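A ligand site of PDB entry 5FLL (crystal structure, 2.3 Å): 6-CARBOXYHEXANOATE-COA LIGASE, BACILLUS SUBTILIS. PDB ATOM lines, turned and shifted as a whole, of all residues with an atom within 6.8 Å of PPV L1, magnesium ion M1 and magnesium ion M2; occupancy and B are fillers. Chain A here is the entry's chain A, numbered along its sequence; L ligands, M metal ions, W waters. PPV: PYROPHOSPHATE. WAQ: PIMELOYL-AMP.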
ATOM      1  N   MET A  13      17.112   6.698  -7.744  1.00  0.00           N
ATOM      2  CA  MET A  13      17.747   7.753  -8.475  1.00  0.00           C
ATOM      3  C   MET A  13      18.677   8.505  -7.537  1.00  0.00           C
ATOM      4  O   MET A  13      18.384   8.699  -6.360  1.00  0.00           O
ATOM      5  CB  MET A  13      16.671   8.712  -9.020  1.00  0.00           C
ATOM      6  CG  MET A  13      17.202   9.934  -9.774  1.00  0.00           C
ATOM      7  SD  MET A  13      17.559  11.322  -8.687  1.00  0.00           S
ATOM      8  CE  MET A  13      15.932  11.839  -8.196  1.00  0.00           C
ATOM      9  N   HIS A  27      25.438  17.004  -3.861  1.00  0.00           N
ATOM     10  CA  HIS A  27      24.233  16.194  -3.969  1.00  0.00           C
ATOM     11  C   HIS A  27      23.067  17.107  -4.269  1.00  0.00           C
ATOM     12  O   HIS A  27      22.913  18.169  -3.651  1.00  0.00           O
ATOM     13  CB  HIS A  27      23.981  15.464  -2.659  1.00  0.00           C
ATOM     14  CG  HIS A  27      22.649  14.812  -2.583  1.00  0.00           C
ATOM     15  ND1 HIS A  27      22.346  13.673  -3.287  1.00  0.00           N
ATOM     16  CD2 HIS A  27      21.536  15.116  -1.861  1.00  0.00           C
ATOM     17  CE1 HIS A  27      21.104  13.288  -2.996  1.00  0.00           C
ATOM     18  NE2 HIS A  27      20.604  14.138  -2.112  1.00  0.00           N
ATOM     19  N   ILE A  28      22.292  16.737  -5.267  1.00  0.00           N
ATOM     20  CA  ILE A  28      21.171  17.567  -5.682  1.00  0.00           C
ATOM     21  C   ILE A  28      19.899  16.884  -5.268  1.00  0.00           C
ATOM     22  O   ILE A  28      19.050  17.495  -4.585  1.00  0.00           O
ATOM     23  CB  ILE A  28      21.113  17.753  -7.215  1.00  0.00           C
ATOM     24  CG1 ILE A  28      22.316  18.541  -7.733  1.00  0.00           C
ATOM     25  CG2 ILE A  28      19.799  18.422  -7.604  1.00  0.00           C
ATOM     26  CD1 ILE A  28      22.250  20.010  -7.388  1.00  0.00           C
ATOM     27  N   SER A  29      19.756  15.625  -5.681  1.00  0.00           N
ATOM     28  CA  SER A  29      18.489  14.928  -5.432  1.00  0.00           C
ATOM     29  C   SER A  29      18.669  13.434  -5.302  1.00  0.00           C
ATOM     30  O   SER A  29      19.567  12.849  -5.909  1.00  0.00           O
ATOM     31  CB  SER A  29      17.462  15.234  -6.540  1.00  0.00           C
ATOM     32  OG  SER A  29      16.231  14.545  -6.260  1.00  0.00           O
ATOM     33  N   GLY A  30      17.784  12.817  -4.516  1.00  0.00           N
ATOM     34  CA  GLY A  30      17.742  11.378  -4.367  1.00  0.00           C
ATOM     35  C   GLY A  30      16.302  10.924  -4.342  1.00  0.00           C
ATOM     36  O   GLY A  30      15.416  11.626  -3.837  1.00  0.00           O
ATOM     37  N   GLY A  31      16.072   9.732  -4.843  1.00  0.00           N
ATOM     38  CA  GLY A  31      14.750   9.158  -4.818  1.00  0.00           C
ATOM     39  C   GLY A  31      14.761   7.654  -4.708  1.00  0.00           C
ATOM     40  O   GLY A  31      15.678   6.973  -5.184  1.00  0.00           O
ATOM     41  N   GLU A  32      13.673   7.132  -4.137  1.00  0.00           N
ATOM     42  CA  GLU A  32      13.454   5.701  -4.017  1.00  0.00           C
ATOM     43  C   GLU A  32      11.954   5.384  -4.168  1.00  0.00           C
ATOM     44  O   GLU A  32      11.088   6.082  -3.621  1.00  0.00           O
ATOM     45  CB  GLU A  32      13.991   5.187  -2.676  1.00  0.00           C
ATOM     46  CG  GLU A  32      13.758   6.157  -1.531  1.00  0.00           C
ATOM     47  CD  GLU A  32      14.900   7.148  -1.375  1.00  0.00           C
ATOM     48  OE1 GLU A  32      16.062   6.790  -1.630  1.00  0.00           O
ATOM     49  OE2 GLU A  32      14.632   8.296  -0.959  1.00  0.00           O
ATOM     50  N   LYS A  50      12.111  14.843 -11.204  1.00  0.00           N
ATOM     51  CA  LYS A  50      12.444  15.255  -9.845  1.00  0.00           C
ATOM     52  C   LYS A  50      13.886  15.703  -9.746  1.00  0.00           C
ATOM     53  O   LYS A  50      14.175  16.757  -9.199  1.00  0.00           O
ATOM     54  CB  LYS A  50      12.192  14.110  -8.888  1.00  0.00           C
ATOM     55  CG  LYS A  50      12.675  14.293  -7.463  1.00  0.00           C
ATOM     56  CD  LYS A  50      12.315  13.065  -6.650  1.00  0.00           C
ATOM     57  CE  LYS A  50      12.960  13.053  -5.270  1.00  0.00           C
ATOM     58  NZ  LYS A  50      12.190  13.879  -4.288  1.00  0.00           N
ATOM     59  N   GLY A  51      14.786  14.917 -10.303  1.00  0.00           N
ATOM     60  CA  GLY A  51      16.177  15.279 -10.334  1.00  0.00           C
ATOM     61  C   GLY A  51      16.502  16.529 -11.131  1.00  0.00           C
ATOM     62  O   GLY A  51      17.415  17.280 -10.750  1.00  0.00           O
ATOM     63  N   HIS A  54      15.312  20.426  -9.626  1.00  0.00           N
ATOM     64  CA  HIS A  54      15.522  20.599  -8.207  1.00  0.00           C
ATOM     65  C   HIS A  54      15.998  22.008  -7.879  1.00  0.00           C
ATOM     66  O   HIS A  54      16.804  22.581  -8.589  1.00  0.00           O
ATOM     67  CB  HIS A  54      16.515  19.563  -7.659  1.00  0.00           C
ATOM     68  CG  HIS A  54      16.360  19.293  -6.206  1.00  0.00           C
ATOM     69  ND1 HIS A  54      16.784  20.177  -5.240  1.00  0.00           N
ATOM     70  CD2 HIS A  54      15.794  18.249  -5.545  1.00  0.00           C
ATOM     71  CE1 HIS A  54      16.496  19.690  -4.042  1.00  0.00           C
ATOM     72  NE2 HIS A  54      15.901  18.515  -4.201  1.00  0.00           N
ATOM     73  N   ARG A  56      17.988  22.920  -5.510  1.00  0.00           N
ATOM     74  CA  ARG A  56      19.425  22.925  -5.258  1.00  0.00           C
ATOM     75  C   ARG A  56      20.254  23.073  -6.553  1.00  0.00           C
ATOM     76  O   ARG A  56      21.436  23.379  -6.482  1.00  0.00           O
ATOM     77  CB  ARG A  56      19.850  21.666  -4.522  1.00  0.00           C
ATOM     78  CG  ARG A  56      19.390  21.625  -3.063  1.00  0.00           C
ATOM     79  CD  ARG A  56      19.566  20.263  -2.406  1.00  0.00           C
ATOM     80  NE  ARG A  56      20.982  19.896  -2.266  1.00  0.00           N
ATOM     81  CZ  ARG A  56      21.765  20.250  -1.244  1.00  0.00           C
ATOM     82  NH1 ARG A  56      21.304  21.002  -0.240  1.00  0.00           N
ATOM     83  NH2 ARG A  56      23.038  19.877  -1.258  1.00  0.00           N
ATOM     84  N   ARG A 124      24.386  12.551   2.522  1.00  0.00           N
ATOM     85  CA  ARG A 124      23.456  12.290   1.416  1.00  0.00           C
ATOM     86  C   ARG A 124      22.317  11.375   1.797  1.00  0.00           C
ATOM     87  O   ARG A 124      21.275  11.341   1.122  1.00  0.00           O
ATOM     88  CB  ARG A 124      24.241  11.712   0.258  1.00  0.00           C
ATOM     89  CG  ARG A 124      25.500  12.522   0.026  1.00  0.00           C
ATOM     90  CD  ARG A 124      25.976  12.491  -1.401  1.00  0.00           C
ATOM     91  NE  ARG A 124      26.633  11.223  -1.716  1.00  0.00           N
ATOM     92  CZ  ARG A 124      27.880  10.916  -1.368  1.00  0.00           C
ATOM     93  NH1 ARG A 124      28.617  11.765  -0.648  1.00  0.00           N
ATOM     94  NH2 ARG A 124      28.381   9.737  -1.714  1.00  0.00           N
ATOM     95  N   GLY A 125      22.503  10.628   2.878  1.00  0.00           N
ATOM     96  CA  GLY A 125      21.430   9.845   3.479  1.00  0.00           C
ATOM     97  C   GLY A 125      21.194  10.274   4.926  1.00  0.00           C
ATOM     98  O   GLY A 125      21.183  11.456   5.243  1.00  0.00           O
ATOM     99  N   ARG A 146      21.049   5.224   3.341  1.00  0.00           N
ATOM    100  CA  ARG A 146      19.927   5.544   2.483  1.00  0.00           C
ATOM    101  C   ARG A 146      18.849   4.478   2.621  1.00  0.00           C
ATOM    102  O   ARG A 146      19.009   3.361   2.178  1.00  0.00           O
ATOM    103  CB  ARG A 146      20.373   5.679   1.030  1.00  0.00           C
ATOM    104  CG  ARG A 146      19.348   6.391   0.153  1.00  0.00           C
ATOM    105  CD  ARG A 146      19.351   7.907   0.314  1.00  0.00           C
ATOM    106  NE  ARG A 146      18.184   8.497  -0.377  1.00  0.00           N
ATOM    107  CZ  ARG A 146      17.942   9.809  -0.546  1.00  0.00           C
ATOM    108  NH1 ARG A 146      18.763  10.725  -0.066  1.00  0.00           N
ATOM    109  NH2 ARG A 146      16.859  10.190  -1.211  1.00  0.00           N
ATOM    110  N   ARG A 171       6.226  15.417  -1.598  1.00  0.00           N
ATOM    111  CA  ARG A 171       7.236  15.601  -0.576  1.00  0.00           C
ATOM    112  C   ARG A 171       6.790  15.027   0.774  1.00  0.00           C
ATOM    113  O   ARG A 171       7.585  14.573   1.599  1.00  0.00           O
ATOM    114  CB  ARG A 171       7.491  17.091  -0.465  1.00  0.00           C
ATOM    115  CG  ARG A 171       8.824  17.453   0.112  1.00  0.00           C
ATOM    116  CD  ARG A 171       8.786  18.875   0.593  1.00  0.00           C
ATOM    117  NE  ARG A 171       9.128  19.844  -0.431  1.00  0.00           N
ATOM    118  CZ  ARG A 171      10.379  20.165  -0.770  1.00  0.00           C
ATOM    119  NH1 ARG A 171      11.402  19.532  -0.183  1.00  0.00           N
ATOM    120  NH2 ARG A 171      10.600  21.114  -1.674  1.00  0.00           N
ATOM    121  N   GLU A 174       6.597  11.219   0.494  1.00  0.00           N
ATOM    122  CA  GLU A 174       7.905  10.594   0.571  1.00  0.00           C
ATOM    123  C   GLU A 174       8.443  10.614   1.989  1.00  0.00           C
ATOM    124  O   GLU A 174       8.901   9.580   2.499  1.00  0.00           O
ATOM    125  CB  GLU A 174       8.867  11.259  -0.414  1.00  0.00           C
ATOM    126  CG  GLU A 174       8.473  10.974  -1.854  1.00  0.00           C
ATOM    127  CD  GLU A 174       9.180  11.846  -2.880  1.00  0.00           C
ATOM    128  OE1 GLU A 174      10.017  12.689  -2.483  1.00  0.00           O
ATOM    129  OE2 GLU A 174       8.850  11.710  -4.087  1.00  0.00           O
ATOM    130  N   ALA A 175       8.323  11.766   2.645  1.00  0.00           N
ATOM    131  CA  ALA A 175       8.772  11.897   4.033  1.00  0.00           C
ATOM    132  C   ALA A 175       8.049  10.946   4.959  1.00  0.00           C
ATOM    133  O   ALA A 175       8.662  10.366   5.867  1.00  0.00           O
ATOM    134  CB  ALA A 175       8.580  13.318   4.534  1.00  0.00           C
ATOM    135  N   SER A 195      14.528  19.504   5.569  1.00  0.00           N
ATOM    136  CA  SER A 195      15.013  19.373   4.210  1.00  0.00           C
ATOM    137  C   SER A 195      16.307  20.134   3.981  1.00  0.00           C
ATOM    138  O   SER A 195      16.554  21.181   4.579  1.00  0.00           O
ATOM    139  CB  SER A 195      13.932  19.836   3.218  1.00  0.00           C
ATOM    140  OG  SER A 195      14.350  19.547   1.889  1.00  0.00           O
ATOM    141  N   ASP A 196      17.139  19.600   3.091  1.00  0.00           N
ATOM    142  CA  ASP A 196      18.282  20.334   2.569  1.00  0.00           C
ATOM    143  C   ASP A 196      17.895  21.253   1.404  1.00  0.00           C
ATOM    144  O   ASP A 196      18.765  21.900   0.810  1.00  0.00           O
ATOM    145  CB  ASP A 196      19.407  19.368   2.160  1.00  0.00           C
ATOM    146  CG  ASP A 196      18.995  18.402   1.070  1.00  0.00           C
ATOM    147  OD1 ASP A 196      17.812  18.022   0.997  1.00  0.00           O
ATOM    148  OD2 ASP A 196      19.875  18.007   0.257  1.00  0.00           O
ATOM    149  N   ASP A 197      16.601  21.315   1.056  1.00  0.00           N
ATOM    150  CA  ASP A 197      16.207  22.152  -0.101  1.00  0.00           C
ATOM    151  C   ASP A 197      16.031  23.612   0.319  1.00  0.00           C
ATOM    152  O   ASP A 197      15.466  23.897   1.356  1.00  0.00           O
ATOM    153  CB  ASP A 197      14.919  21.629  -0.742  1.00  0.00           C
ATOM    154  CG  ASP A 197      14.936  20.120  -1.008  1.00  0.00           C
ATOM    155  OD1 ASP A 197      15.979  19.439  -0.907  1.00  0.00           O
ATOM    156  OD2 ASP A 197      13.850  19.598  -1.293  1.00  0.00           O
ATOM    157  N   ARG A 228      18.950  14.675   8.827  1.00  0.00           N
ATOM    158  CA  ARG A 228      18.254  13.395   8.939  1.00  0.00           C
ATOM    159  C   ARG A 228      19.053  12.528   9.896  1.00  0.00           C
ATOM    160  O   ARG A 228      20.085  11.957   9.529  1.00  0.00           O
ATOM    161  CB  ARG A 228      18.151  12.716   7.561  1.00  0.00           C
ATOM    162  CG  ARG A 228      16.884  11.918   7.306  1.00  0.00           C
ATOM    163  CD  ARG A 228      15.712  12.865   7.312  1.00  0.00           C
ATOM    164  NE  ARG A 228      14.421  12.288   6.978  1.00  0.00           N
ATOM    165  CZ  ARG A 228      13.826  12.441   5.804  1.00  0.00           C
ATOM    166  NH1 ARG A 228      14.451  13.051   4.793  1.00  0.00           N
ATOM    167  NH2 ARG A 228      12.597  11.982   5.643  1.00  0.00           N
HETATM  168  O11 PPV L   1      18.180  13.400  -1.275  1.00  0.00           O
HETATM  169  P1  PPV L   1      16.861  14.071  -0.998  1.00  0.00           P
HETATM  170  O21 PPV L   1      15.752  13.147  -0.583  1.00  0.00           O
HETATM  171  O31 PPV L   1      16.932  15.364  -0.175  1.00  0.00           O
HETATM  172  OPP PPV L   1      16.350  14.503  -2.494  1.00  0.00           O
HETATM  173  P2  PPV L   1      15.035  15.424  -2.733  1.00  0.00           P
HETATM  174  O12 PPV L   1      13.880  14.716  -2.061  1.00  0.00           O
HETATM  175  O22 PPV L   1      14.874  15.471  -4.234  1.00  0.00           O
HETATM  176  O32 PPV L   1      15.373  16.737  -2.036  1.00  0.00           O
HETATM  177  N1  WAQ L   2      17.250   7.634   3.459  1.00  0.00           N
HETATM  178  C2  WAQ L   2      18.085   8.267   4.387  1.00  0.00           C
HETATM  179  N3  WAQ L   2      18.152   9.656   4.410  1.00  0.00           N
HETATM  180  C4  WAQ L   2      17.423  10.351   3.511  1.00  0.00           C
HETATM  181  C5  WAQ L   2      16.604   9.732   2.637  1.00  0.00           C
HETATM  182  C6  WAQ L   2      16.544   8.388   2.604  1.00  0.00           C
HETATM  183  N6  WAQ L   2      15.748   7.825   1.710  1.00  0.00           N
HETATM  184  N7  WAQ L   2      15.994  10.673   1.903  1.00  0.00           N
HETATM  185  C8  WAQ L   2      16.408  11.864   2.307  1.00  0.00           C
HETATM  186  N9  WAQ L   2      17.292  11.664   3.314  1.00  0.00           N
HETATM  187  C1' WAQ L   2      18.066  12.654   4.054  1.00  0.00           C
HETATM  188  C2' WAQ L   2      19.114  13.195   3.116  1.00  0.00           C
HETATM  189  O2' WAQ L   2      20.240  13.634   3.837  1.00  0.00           O
HETATM  190  C3' WAQ L   2      18.429  14.427   2.535  1.00  0.00           C
HETATM  191  O3' WAQ L   2      19.368  15.337   1.972  1.00  0.00           O
HETATM  192  C4' WAQ L   2      17.818  14.973   3.785  1.00  0.00           C
HETATM  193  O4' WAQ L   2      17.340  13.800   4.502  1.00  0.00           O
HETATM  194  C5' WAQ L   2      16.588  15.824   3.439  1.00  0.00           C
HETATM  195  O5' WAQ L   2      15.964  15.160   2.409  1.00  0.00           O
HETATM  196  OAB WAQ L   2       5.709  18.699   5.131  1.00  0.00           O
HETATM  197  OAC WAQ L   2      11.776  16.968   2.013  1.00  0.00           O
HETATM  198  OAD WAQ L   2      15.006  17.171   1.072  1.00  0.00           O
HETATM  199  OAE WAQ L   2       5.235  16.772   6.266  1.00  0.00           O
HETATM  200  OAH WAQ L   2      13.965  14.769   0.852  1.00  0.00           O
HETATM  201  CAK WAQ L   2       9.726  16.901   5.817  1.00  0.00           C
HETATM  202  CAL WAQ L   2       8.352  17.623   5.933  1.00  0.00           C
HETATM  203  CAM WAQ L   2      10.374  17.173   4.472  1.00  0.00           C
HETATM  204  CAN WAQ L   2       7.314  16.958   5.059  1.00  0.00           C
HETATM  205  CAO WAQ L   2      11.833  16.757   4.485  1.00  0.00           C
HETATM  206  OAU WAQ L   2      13.677  16.129   3.044  1.00  0.00           O
HETATM  207  CAW WAQ L   2       5.986  17.528   5.538  1.00  0.00           C
HETATM  208  CAX WAQ L   2      12.400  16.608   3.031  1.00  0.00           C
HETATM  209  PBG WAQ L   2      14.582  15.768   1.786  1.00  0.00           P
HETATM  210 MG    MG M   1      13.698  13.218  -0.688  1.00  0.00          MG
HETATM  211 MG    MG M   2      16.427  17.477  -0.555  1.00  0.00          MG
HETATM  212  O   HOH W   1      18.213  17.413  -1.786  1.00  0.00           O
HETATM  213  O   HOH W   2      13.490  11.578   0.903  1.00  0.00           O
HETATM  214  O   HOH W   3      12.474  17.067  -1.053  1.00  0.00           O
HETATM  215  O   HOH W   4      12.802  16.488  -5.064  1.00  0.00           O
HETATM  216  O   HOH W   5      13.407  11.732  -2.084  1.00  0.00           O
HETATM  217  O   HOH W   6      11.638  13.444  -0.529  1.00  0.00           O
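An oxygen (O22) of PPV L1 is in hydrogen-bond range of the side-chain hydroxyl (OG) of Ser 29, at 2.6 Å. NE2 of His 27 sits at hydrogen-bond distance from O11 of PPV L1 (2.7 Å). O22 of PPV L1 lies close to NE2 of His 54 (3.2 Å). An oxygen (O22) of PPV L1 lies within salt-bridge range of the side-chain amino group (NZ) of Lys 50 (3.1 Å). O11 of PPV L1 lies within salt-bridge range of NH1 of Arg 146 (3.0 Å). The backbone NH of Gly 30 sits at hydrogen-bond distance from an oxygen (OPP) of PPV L1 (3.0 Å). The guanidinium group (NH2) of Arg 146 sits close to a nitrogen (N7) of WAQ L2 (3.3 Å). The side-chain hydroxyl of Ser 195 sits close to an oxygen (OAD) of WAQ L2, 2.6 Å away. A nitrogen (N6) of WAQ L2 is in hydrogen-bond range of the side-chain carboxylate (OE2) of Glu 32, 2.9 Å away. The guanidinium group of Arg 171 lies within hydrogen-bond range of an oxygen (OAC) of WAQ L2, 3.4 Å away. NH1 of Arg 228 sits at hydrogen-bond distance from O4' of WAQ L2. O of Gly 125 is in hydrogen-bond range of O2' of WAQ L2, at 2.8 Å.
Gly 30 touches magnesium ion M1 (O to MG, 3.9 Å). NZ of Lys 50 touches magnesium ion M1 (3.96 Å). Of the 21 residues printed, 2 come within 4 Å of magnesium ion M1. Along chain A the residues within 4 Å of magnesium ion M1 span positions 30 to 50.
Water W5 lies within hydrogen-bond range of the backbone carbonyl oxygen of Gly 30 (2.7 Å) and the side-chain amino group of Lys 50 (3.3 Å). Water W1 bridges the side-chain carboxylate of Asp 196 (2.7 Å) and the backbone carbonyl oxygen of Ile 28 (2.9 Å). Water W4 lies within hydrogen-bond range of O22 of PPV L1 and NZ of Lys 50. Water W3 lies within hydrogen-bond range of NH1 of Arg 171, OD2 of Asp 197 and OAC of WAQ L2.
NE2 of His 54 touches magnesium ion M2, at 3.8 Å. Ser 195 touches magnesium ion M2. Of the 21 residues printed, 4 come within 4 Å of magnesium ion M2. The nearest printed residue that does not touch magnesium ion M2 is Arg 56 (4.6 Å).
Of the 21 residues printed, 8 come within 4 Å of PPV L1.
Magnesium ion M1 is bound by O12 of PPV L1 (2.0 Å), O21 of PPV L1 (2.1 Å), water W5 (2.1 Å), water W6 (2.1 Å), OAH of WAQ L2 (2.2 Å) and water W2 (2.3 Å). Magnesium ion M1 has six donor atoms within binding distance.
OD1 of Asp 197 sits close to NE2 of His 54. The side-chain carboxylate (OD2) of Asp 197 is in salt-bridge range of the guanidinium group (NH1) of Arg 171 (2.7 Å). The side-chain carboxylate of Asp 196 is in salt-bridge range of the guanidinium group of Arg 56 (3.3 Å). O of His 27 lies within hydrogen-bond range of NE of Arg 56, 2.9 Å away. The side-chain carboxylate (OE1) of Glu 174 lies within salt-bridge range of the side-chain amino group (NZ) of Lys 50 (3.1 Å). NH2 of Arg 146 lies close to O of Gly 30 (3.3 Å). O of Arg 124 lies within hydrogen-bond range of NH1 of Arg 146 (2.8 Å). The guanidinium group of Arg 146 is in salt-bridge range of the side-chain carboxylate of Glu 32 (2.9 Å).
Magnesium ion M2 is bound by an oxygen (O32) of PPV L1, the side-chain carboxylate (OD1) of Asp 197, the side-chain carboxylate (OD1) of Asp 196, water W1, an oxygen (OAD) of WAQ L2 and an oxygen (O31) of PPV L1.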
